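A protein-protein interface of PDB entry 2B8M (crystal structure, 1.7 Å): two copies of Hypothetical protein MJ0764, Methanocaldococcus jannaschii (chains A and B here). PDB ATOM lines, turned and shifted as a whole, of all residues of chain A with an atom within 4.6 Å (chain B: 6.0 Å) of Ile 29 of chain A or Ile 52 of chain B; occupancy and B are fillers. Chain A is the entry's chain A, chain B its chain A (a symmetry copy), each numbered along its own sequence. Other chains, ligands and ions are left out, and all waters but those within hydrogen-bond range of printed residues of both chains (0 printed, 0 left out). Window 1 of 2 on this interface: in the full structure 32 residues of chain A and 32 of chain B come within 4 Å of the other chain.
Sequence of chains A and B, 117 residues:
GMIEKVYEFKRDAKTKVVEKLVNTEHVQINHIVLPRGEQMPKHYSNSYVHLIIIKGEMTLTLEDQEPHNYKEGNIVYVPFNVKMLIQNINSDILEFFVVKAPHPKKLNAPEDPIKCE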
ATOM      1  N   PHE A   9      12.930 -17.863  26.388  1.00  0.00           N
ATOM      2  CA  PHE A   9      11.941 -18.799  25.903  1.00  0.00           C
ATOM      3  C   PHE A   9      12.594 -19.722  24.873  1.00  0.00           C
ATOM      4  O   PHE A   9      13.539 -19.332  24.156  1.00  0.00           O
ATOM      5  CB  PHE A   9      10.671 -18.101  25.390  1.00  0.00           C
ATOM      6  CG  PHE A   9      10.835 -17.278  24.104  1.00  0.00           C
ATOM      7  CD1 PHE A   9      10.779 -17.878  22.852  1.00  0.00           C
ATOM      8  CD2 PHE A   9      10.999 -15.912  24.171  1.00  0.00           C
ATOM      9  CE1 PHE A   9      10.890 -17.114  21.698  1.00  0.00           C
ATOM     10  CE2 PHE A   9      11.142 -15.143  23.015  1.00  0.00           C
ATOM     11  CZ  PHE A   9      11.082 -15.747  21.789  1.00  0.00           C
ATOM     12  N   GLU A  19       5.790 -22.756  28.958  1.00  0.00           N
ATOM     13  CA  GLU A  19       6.723 -21.935  29.714  1.00  0.00           C
ATOM     14  C   GLU A  19       6.040 -20.755  30.393  1.00  0.00           C
ATOM     15  O   GLU A  19       5.705 -19.757  29.744  1.00  0.00           O
ATOM     16  CB  GLU A  19       7.855 -21.415  28.802  1.00  0.00           C
ATOM     17  CG  GLU A  19       8.653 -22.511  28.226  1.00  0.00           C
ATOM     18  CD  GLU A  19       9.824 -22.055  27.394  1.00  0.00           C
ATOM     19  OE1 GLU A  19       9.635 -21.246  26.444  1.00  0.00           O
ATOM     20  OE2 GLU A  19      10.911 -22.593  27.638  1.00  0.00           O
ATOM     21  N   LYS A  20       5.881 -20.875  31.708  1.00  0.00           N
ATOM     22  CA  LYS A  20       5.244 -19.845  32.512  1.00  0.00           C
ATOM     23  C   LYS A  20       6.337 -18.947  33.008  1.00  0.00           C
ATOM     24  O   LYS A  20       6.890 -19.157  34.069  1.00  0.00           O
ATOM     25  CB  LYS A  20       4.474 -20.492  33.640  1.00  0.00           C
ATOM     26  CG  LYS A  20       3.294 -21.297  33.068  1.00  0.00           C
ATOM     27  CD  LYS A  20       2.395 -21.858  34.145  1.00  0.00           C
ATOM     28  CE  LYS A  20       1.306 -20.861  34.560  1.00  0.00           C
ATOM     29  NZ  LYS A  20       0.581 -21.273  35.806  1.00  0.00           N
ATOM     30  N   LEU A  21       6.676 -17.965  32.179  1.00  0.00           N
ATOM     31  CA  LEU A  21       7.924 -17.238  32.351  1.00  0.00           C
ATOM     32  C   LEU A  21       7.823 -16.023  33.217  1.00  0.00           C
ATOM     33  O   LEU A  21       8.575 -15.912  34.192  1.00  0.00           O
ATOM     34  CB  LEU A  21       8.491 -16.862  30.995  1.00  0.00           C
ATOM     35  CG  LEU A  21       9.114 -18.066  30.241  1.00  0.00           C
ATOM     36  CD1 LEU A  21       9.325 -17.614  28.809  1.00  0.00           C
ATOM     37  CD2 LEU A  21      10.377 -18.589  30.866  1.00  0.00           C
ATOM     38  N   VAL A  22       6.932 -15.105  32.867  1.00  0.00           N
ATOM     39  CA  VAL A  22       6.774 -13.824  33.543  1.00  0.00           C
ATOM     40  C   VAL A  22       5.518 -13.898  34.405  1.00  0.00           C
ATOM     41  O   VAL A  22       4.440 -14.283  33.908  1.00  0.00           O
ATOM     42  CB  VAL A  22       6.640 -12.663  32.547  1.00  0.00           C
ATOM     43  CG1 VAL A  22       6.418 -11.322  33.274  1.00  0.00           C
ATOM     44  CG2 VAL A  22       7.862 -12.572  31.653  1.00  0.00           C
ATOM     45  N   VAL A  27       1.410  -8.387  35.435  1.00  0.00           N
ATOM     46  CA  VAL A  27       1.245  -9.106  34.166  1.00  0.00           C
ATOM     47  C   VAL A  27       1.768 -10.537  34.277  1.00  0.00           C
ATOM     48  O   VAL A  27       2.658 -10.830  35.059  1.00  0.00           O
ATOM     49  CB  VAL A  27       1.965  -8.405  32.961  1.00  0.00           C
ATOM     50  CG1 VAL A  27       3.469  -8.695  32.967  1.00  0.00           C
ATOM     51  CG2 VAL A  27       1.413  -8.809  31.595  1.00  0.00           C
ATOM     52  N   GLN A  28       1.214 -11.412  33.444  1.00  0.00           N
ATOM     53  CA  GLN A  28       1.750 -12.738  33.209  1.00  0.00           C
ATOM     54  C   GLN A  28       1.999 -12.925  31.715  1.00  0.00           C
ATOM     55  O   GLN A  28       1.194 -12.520  30.864  1.00  0.00           O
ATOM     56  CB  GLN A  28       0.843 -13.841  33.728  1.00  0.00           C
ATOM     57  CG  GLN A  28       0.576 -13.814  35.167  1.00  0.00           C
ATOM     58  CD  GLN A  28      -0.478 -14.833  35.567  1.00  0.00           C
ATOM     59  OE1 GLN A  28      -1.544 -14.942  34.934  1.00  0.00           O
ATOM     60  NE2 GLN A  28      -0.197 -15.588  36.612  1.00  0.00           N
ATOM     61  N   ILE A  29       3.153 -13.500  31.392  1.00  0.00           N
ATOM     62  CA  ILE A  29       3.484 -13.814  30.014  1.00  0.00           C
ATOM     63  C   ILE A  29       4.012 -15.240  29.950  1.00  0.00           C
ATOM     64  O   ILE A  29       5.021 -15.581  30.563  1.00  0.00           O
ATOM     65  CB  ILE A  29       4.504 -12.808  29.392  1.00  0.00           C
ATOM     66  CG1 ILE A  29       4.050 -11.350  29.577  1.00  0.00           C
ATOM     67  CG2 ILE A  29       4.720 -13.135  27.902  1.00  0.00           C
ATOM     68  CD1 ILE A  29       5.011 -10.325  29.082  1.00  0.00           C
ATOM     69  N   ASN A  30       3.325 -16.077  29.185  1.00  0.00           N
ATOM     70  CA  ASN A  30       3.717 -17.465  28.967  1.00  0.00           C
ATOM     71  C   ASN A  30       4.046 -17.696  27.503  1.00  0.00           C
ATOM     72  O   ASN A  30       3.558 -16.978  26.625  1.00  0.00           O
ATOM     73  CB  ASN A  30       2.599 -18.403  29.458  1.00  0.00           C
ATOM     74  CG  ASN A  30       2.203 -18.121  30.861  1.00  0.00           C
ATOM     75  OD1 ASN A  30       3.044 -17.731  31.687  1.00  0.00           O
ATOM     76  ND2 ASN A  30       0.931 -18.308  31.175  1.00  0.00           N
ATOM     77  N   HIS A  31       4.881 -18.713  27.243  1.00  0.00           N
ATOM     78  CA  HIS A  31       5.234 -19.121  25.911  1.00  0.00           C
ATOM     79  C   HIS A  31       4.824 -20.575  25.739  1.00  0.00           C
ATOM     80  O   HIS A  31       5.185 -21.426  26.542  1.00  0.00           O
ATOM     81  CB  HIS A  31       6.709 -18.948  25.709  1.00  0.00           C
ATOM     82  CG  HIS A  31       7.214 -19.524  24.423  1.00  0.00           C
ATOM     83  ND1 HIS A  31       8.077 -20.587  24.393  1.00  0.00           N
ATOM     84  CD2 HIS A  31       6.955 -19.202  23.136  1.00  0.00           C
ATOM     85  CE1 HIS A  31       8.360 -20.880  23.133  1.00  0.00           C
ATOM     86  NE2 HIS A  31       7.706 -20.043  22.352  1.00  0.00           N
ATOM     87  N   PHE A  97       2.405 -16.703  22.386  1.00  0.00           N
ATOM     88  CA  PHE A  97       2.524 -16.144  23.712  1.00  0.00           C
ATOM     89  C   PHE A  97       1.166 -15.849  24.285  1.00  0.00           C
ATOM     90  O   PHE A  97       0.245 -15.501  23.557  1.00  0.00           O
ATOM     91  CB  PHE A  97       3.367 -14.872  23.715  1.00  0.00           C
ATOM     92  CG  PHE A  97       4.775 -15.115  23.259  1.00  0.00           C
ATOM     93  CD1 PHE A  97       5.105 -15.074  21.907  1.00  0.00           C
ATOM     94  CD2 PHE A  97       5.762 -15.423  24.188  1.00  0.00           C
ATOM     95  CE1 PHE A  97       6.393 -15.344  21.523  1.00  0.00           C
ATOM     96  CE2 PHE A  97       7.052 -15.667  23.794  1.00  0.00           C
ATOM     97  CZ  PHE A  97       7.365 -15.640  22.476  1.00  0.00           C
ATOM     98  N   VAL A  98       1.086 -15.965  25.602  1.00  0.00           N
ATOM     99  CA  VAL A  98      -0.109 -15.650  26.349  1.00  0.00           C
ATOM    100  C   VAL A  98       0.238 -14.462  27.224  1.00  0.00           C
ATOM    101  O   VAL A  98       1.195 -14.528  27.970  1.00  0.00           O
ATOM    102  CB  VAL A  98      -0.536 -16.809  27.256  1.00  0.00           C
ATOM    103  CG1 VAL A  98      -1.738 -16.452  28.054  1.00  0.00           C
ATOM    104  CG2 VAL A  98      -0.821 -18.067  26.444  1.00  0.00           C
ATOM    105  N   VAL A  99      -0.527 -13.374  27.087  1.00  0.00           N
ATOM    106  CA  VAL A  99      -0.326 -12.178  27.871  1.00  0.00           C
ATOM    107  C   VAL A  99      -1.578 -12.001  28.709  1.00  0.00           C
ATOM    108  O   VAL A  99      -2.697 -12.002  28.202  1.00  0.00           O
ATOM    109  CB  VAL A  99      -0.113 -10.941  26.978  1.00  0.00           C
ATOM    110  CG1 VAL A  99      -0.111  -9.658  27.824  1.00  0.00           C
ATOM    111  CG2 VAL A  99       1.125 -11.091  26.128  1.00  0.00           C
ATOM    112  N   HIS B  50       7.486  -5.213  28.940  1.00  0.00           N
ATOM    113  CA  HIS B  50       8.165  -6.421  28.494  1.00  0.00           C
ATOM    114  C   HIS B  50       8.280  -6.473  26.983  1.00  0.00           C
ATOM    115  O   HIS B  50       7.306  -6.254  26.267  1.00  0.00           O
ATOM    116  CB  HIS B  50       7.490  -7.699  28.999  1.00  0.00           C
ATOM    117  CG  HIS B  50       7.573  -7.885  30.468  1.00  0.00           C
ATOM    118  ND1 HIS B  50       6.687  -7.282  31.334  1.00  0.00           N
ATOM    119  CD2 HIS B  50       8.459  -8.566  31.241  1.00  0.00           C
ATOM    120  CE1 HIS B  50       7.000  -7.627  32.576  1.00  0.00           C
ATOM    121  NE2 HIS B  50       8.093  -8.361  32.548  1.00  0.00           N
ATOM    122  N   LEU B  51       9.499  -6.738  26.548  1.00  0.00           N
ATOM    123  CA  LEU B  51       9.908  -6.739  25.161  1.00  0.00           C
ATOM    124  C   LEU B  51      10.096  -8.206  24.795  1.00  0.00           C
ATOM    125  O   LEU B  51      10.961  -8.873  25.330  1.00  0.00           O
ATOM    126  CB  LEU B  51      11.242  -5.962  24.997  1.00  0.00           C
ATOM    127  CG  LEU B  51      11.164  -4.512  25.474  1.00  0.00           C
ATOM    128  CD1 LEU B  51      12.548  -3.884  25.401  1.00  0.00           C
ATOM    129  CD2 LEU B  51      10.154  -3.745  24.656  1.00  0.00           C
ATOM    130  N   ILE B  52       9.268  -8.717  23.888  1.00  0.00           N
ATOM    131  CA  ILE B  52       9.340 -10.123  23.501  1.00  0.00           C
ATOM    132  C   ILE B  52      10.024 -10.210  22.142  1.00  0.00           C
ATOM    133  O   ILE B  52       9.446  -9.871  21.102  1.00  0.00           O
ATOM    134  CB  ILE B  52       7.921 -10.772  23.445  1.00  0.00           C
ATOM    135  CG1 ILE B  52       7.179 -10.652  24.784  1.00  0.00           C
ATOM    136  CG2 ILE B  52       8.075 -12.217  23.016  1.00  0.00           C
ATOM    137  CD1 ILE B  52       5.698 -10.973  24.712  1.00  0.00           C
ATOM    138  N   ILE B  53      11.263 -10.656  22.140  1.00  0.00           N
ATOM    139  CA  ILE B  53      12.064 -10.586  20.907  1.00  0.00           C
ATOM    140  C   ILE B  53      11.918 -11.861  20.109  1.00  0.00           C
ATOM    141  O   ILE B  53      12.302 -12.939  20.584  1.00  0.00           O
ATOM    142  CB  ILE B  53      13.516 -10.318  21.234  1.00  0.00           C
ATOM    143  CG1 ILE B  53      13.614  -9.069  22.124  1.00  0.00           C
ATOM    144  CG2 ILE B  53      14.339 -10.135  19.953  1.00  0.00           C
ATOM    145  CD1 ILE B  53      14.971  -8.717  22.488  1.00  0.00           C
ATOM    146  N   ILE B  54      11.383 -11.769  18.894  1.00  0.00           N
ATOM    147  CA  ILE B  54      11.197 -12.972  18.094  1.00  0.00           C
ATOM    148  C   ILE B  54      12.088 -13.099  16.875  1.00  0.00           C
ATOM    149  O   ILE B  54      12.137 -14.185  16.308  1.00  0.00           O
ATOM    150  CB  ILE B  54       9.742 -13.200  17.730  1.00  0.00           C
ATOM    151  CG1 ILE B  54       9.216 -12.057  16.878  1.00  0.00           C
ATOM    152  CG2 ILE B  54       8.842 -13.332  19.018  1.00  0.00           C
ATOM    153  CD1 ILE B  54       7.887 -12.500  16.152  1.00  0.00           C
ATOM    154  N   ASN B  74      14.579 -13.983  23.859  1.00  0.00           N
ATOM    155  CA  ASN B  74      14.577 -13.219  25.122  1.00  0.00           C
ATOM    156  C   ASN B  74      13.294 -12.447  25.314  1.00  0.00           C
ATOM    157  O   ASN B  74      12.722 -11.925  24.351  1.00  0.00           O
ATOM    158  CB  ASN B  74      15.722 -12.194  25.171  1.00  0.00           C
ATOM    159  CG  ASN B  74      17.085 -12.807  25.418  1.00  0.00           C
ATOM    160  OD1 ASN B  74      17.998 -12.583  24.611  1.00  0.00           O
ATOM    161  ND2 ASN B  74      17.260 -13.545  26.525  1.00  0.00           N
ATOM    162  N   ILE B  75      12.844 -12.376  26.563  1.00  0.00           N
ATOM    163  CA  ILE B  75      11.858 -11.413  26.976  1.00  0.00           C
ATOM    164  C   ILE B  75      12.569 -10.542  27.973  1.00  0.00           C
ATOM    165  O   ILE B  75      13.162 -11.049  28.926  1.00  0.00           O
ATOM    166  CB  ILE B  75      10.646 -12.075  27.636  1.00  0.00           C
ATOM    167  CG1 ILE B  75       9.975 -13.035  26.682  1.00  0.00           C
ATOM    168  CG2 ILE B  75       9.694 -11.011  28.208  1.00  0.00           C
ATOM    169  CD1 ILE B  75       8.821 -13.769  27.319  1.00  0.00           C
ATOM    170  N   VAL B  76      12.545  -9.244  27.713  1.00  0.00           N
ATOM    171  CA  VAL B  76      13.262  -8.291  28.547  1.00  0.00           C
ATOM    172  C   VAL B  76      12.276  -7.367  29.247  1.00  0.00           C
ATOM    173  O   VAL B  76      11.479  -6.676  28.596  1.00  0.00           O
ATOM    174  CB  VAL B  76      14.272  -7.455  27.736  1.00  0.00           C
ATOM    175  CG1 VAL B  76      15.020  -6.467  28.684  1.00  0.00           C
ATOM    176  CG2 VAL B  76      15.240  -8.312  26.967  1.00  0.00           C
ATOM    177  N   GLU B  95      12.638  -7.949  15.264  1.00  0.00           N
ATOM    178  CA  GLU B  95      11.205  -8.022  15.425  1.00  0.00           C
ATOM    179  C   GLU B  95      10.875  -8.346  16.879  1.00  0.00           C
ATOM    180  O   GLU B  95      11.379  -9.324  17.429  1.00  0.00           O
ATOM    181  CB  GLU B  95      10.606  -9.074  14.478  1.00  0.00           C
ATOM    182  CG  GLU B  95       9.114  -9.030  14.473  1.00  0.00           C
ATOM    183  CD  GLU B  95       8.480 -10.004  13.511  1.00  0.00           C
ATOM    184  OE1 GLU B  95       9.231 -10.722  12.826  1.00  0.00           O
ATOM    185  OE2 GLU B  95       7.226 -10.064  13.451  1.00  0.00           O
ATOM    186  N   PHE B  96      10.013  -7.535  17.488  1.00  0.00           N
ATOM    187  CA  PHE B  96       9.601  -7.755  18.889  1.00  0.00           C
ATOM    188  C   PHE B  96       8.168  -7.313  19.130  1.00  0.00           C
ATOM    189  O   PHE B  96       7.619  -6.515  18.358  1.00  0.00           O
ATOM    190  CB  PHE B  96      10.568  -7.134  19.899  1.00  0.00           C
ATOM    191  CG  PHE B  96      10.772  -5.688  19.738  1.00  0.00           C
ATOM    192  CD1 PHE B  96      11.568  -5.205  18.726  1.00  0.00           C
ATOM    193  CD2 PHE B  96      10.175  -4.786  20.597  1.00  0.00           C
ATOM    194  CE1 PHE B  96      11.771  -3.819  18.576  1.00  0.00           C
ATOM    195  CE2 PHE B  96      10.347  -3.428  20.459  1.00  0.00           C
ATOM    196  CZ  PHE B  96      11.136  -2.934  19.431  1.00  0.00           C
ATOM    197  N   PHE B  97       7.580  -7.842  20.193  1.00  0.00           N
ATOM    198  CA  PHE B  97       6.369  -7.295  20.758  1.00  0.00           C
ATOM    199  C   PHE B  97       6.673  -6.521  22.011  1.00  0.00           C
ATOM    200  O   PHE B  97       7.588  -6.865  22.748  1.00  0.00           O
ATOM    201  CB  PHE B  97       5.347  -8.385  21.065  1.00  0.00           C
ATOM    202  CG  PHE B  97       4.912  -9.127  19.837  1.00  0.00           C
ATOM    203  CD1 PHE B  97       5.629 -10.229  19.376  1.00  0.00           C
ATOM    204  CD2 PHE B  97       3.802  -8.694  19.121  1.00  0.00           C
ATOM    205  CE1 PHE B  97       5.228 -10.856  18.225  1.00  0.00           C
ATOM    206  CE2 PHE B  97       3.395  -9.345  17.986  1.00  0.00           C
ATOM    207  CZ  PHE B  97       4.105 -10.408  17.533  1.00  0.00           C
ATOM    208  N   VAL B  98       5.860  -5.501  22.241  1.00  0.00           N
ATOM    209  CA  VAL B  98       5.937  -4.685  23.428  1.00  0.00           C
ATOM    210  C   VAL B  98       4.646  -4.917  24.188  1.00  0.00           C
ATOM    211  O   VAL B  98       3.582  -4.743  23.627  1.00  0.00           O
ATOM    212  CB  VAL B  98       6.036  -3.194  23.090  1.00  0.00           C
ATOM    213  CG1 VAL B  98       6.065  -2.363  24.322  1.00  0.00           C
ATOM    214  CG2 VAL B  98       7.274  -2.902  22.251  1.00  0.00           C
ATOM    215  N   VAL B  99       4.763  -5.348  25.449  1.00  0.00           N
ATOM    216  CA  VAL B  99       3.618  -5.590  26.297  1.00  0.00           C
ATOM    217  C   VAL B  99       3.723  -4.605  27.445  1.00  0.00           C
ATOM    218  O   VAL B  99       4.746  -4.507  28.118  1.00  0.00           O
ATOM    219  CB  VAL B  99       3.607  -7.031  26.841  1.00  0.00           C
ATOM    220  CG1 VAL B  99       2.506  -7.200  27.898  1.00  0.00           C
ATOM    221  CG2 VAL B  99       3.509  -8.035  25.717  1.00  0.00           C
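Of chain B, only His 50 and Ile 52 come within 4 Å of Ile 29 of chain A.
Ile 52 of chain B touches just these residues of chain A: Ile 29 and Phe 97.
Of the printed residues of chain B, Val 22 of chain A touches His 50.
Of the printed residues of chain A, Ile 53 of chain B touches Phe 9 (3.3 Å).
Printed residues of chain A within 4 Å of Val 99 of chain B: Val 99 (3.6 Å).
CZ of Phe 9 of chain A touches O of Ile 53 of chain B, at 3.3 Å.
Asn 74 of chain B touches Phe 9 of chain A.
Ile 75 of chain B touches Phe 9 of chain A (CG1 to CD2, 3.95 Å).
Val 22 of chain A touches His 50 of chain B.
CE1 of His 50 of chain B touches CG1 of Val 27 of chain A (3.7 Å).
CD1 of Ile 29 of chain A touches CB of His 50 of chain B, 3.6 Å away.
Ile 52 of chain B touches Ile 29 of chain A.
Phe 97 of chain A touches Ile 52 of chain B.
CG1 of Val 99 of chain A touches CG1 of Val 99 of chain B, at 3.6 Å.
Of the 13 printed residues of chain A, 6 touch a printed residue of chain B.
Among the printed residues, no Asp or Glu carboxylate lies within 4 Å of a Lys or Arg side-chain nitrogen of the other chain.
The backbone carbonyl oxygen (O) of Val 22 of chain A sits at hydrogen-bond distance from the backbone NH (N) of Ile 29 of chain A (2.9 Å).
The backbone NH (N) of Val 99 of chain B is in hydrogen-bond range of the backbone carbonyl oxygen (O) of His 50 of chain B (2.8 Å).
The backbone NH (N) of Ile 53 of chain B lies within hydrogen-bond range of the backbone carbonyl oxygen (O) of Asn 74 of chain B (2.9 Å).
N of Leu 21 of chain A is in hydrogen-bond range of O of Ile 29 of chain A (3.3 Å).
The backbone NH of Ile 52 of chain B sits at hydrogen-bond distance from the backbone carbonyl oxygen of Phe 97 of chain B, 2.7 Å away.
Val 99 of chain A touches its own counterpart, Val 99 of chain B.
3 positions are printed for both chains.
Of the 9 pairs that touch across the chains among the printed residues, 1 has its exchanged pair printed and touching as well.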
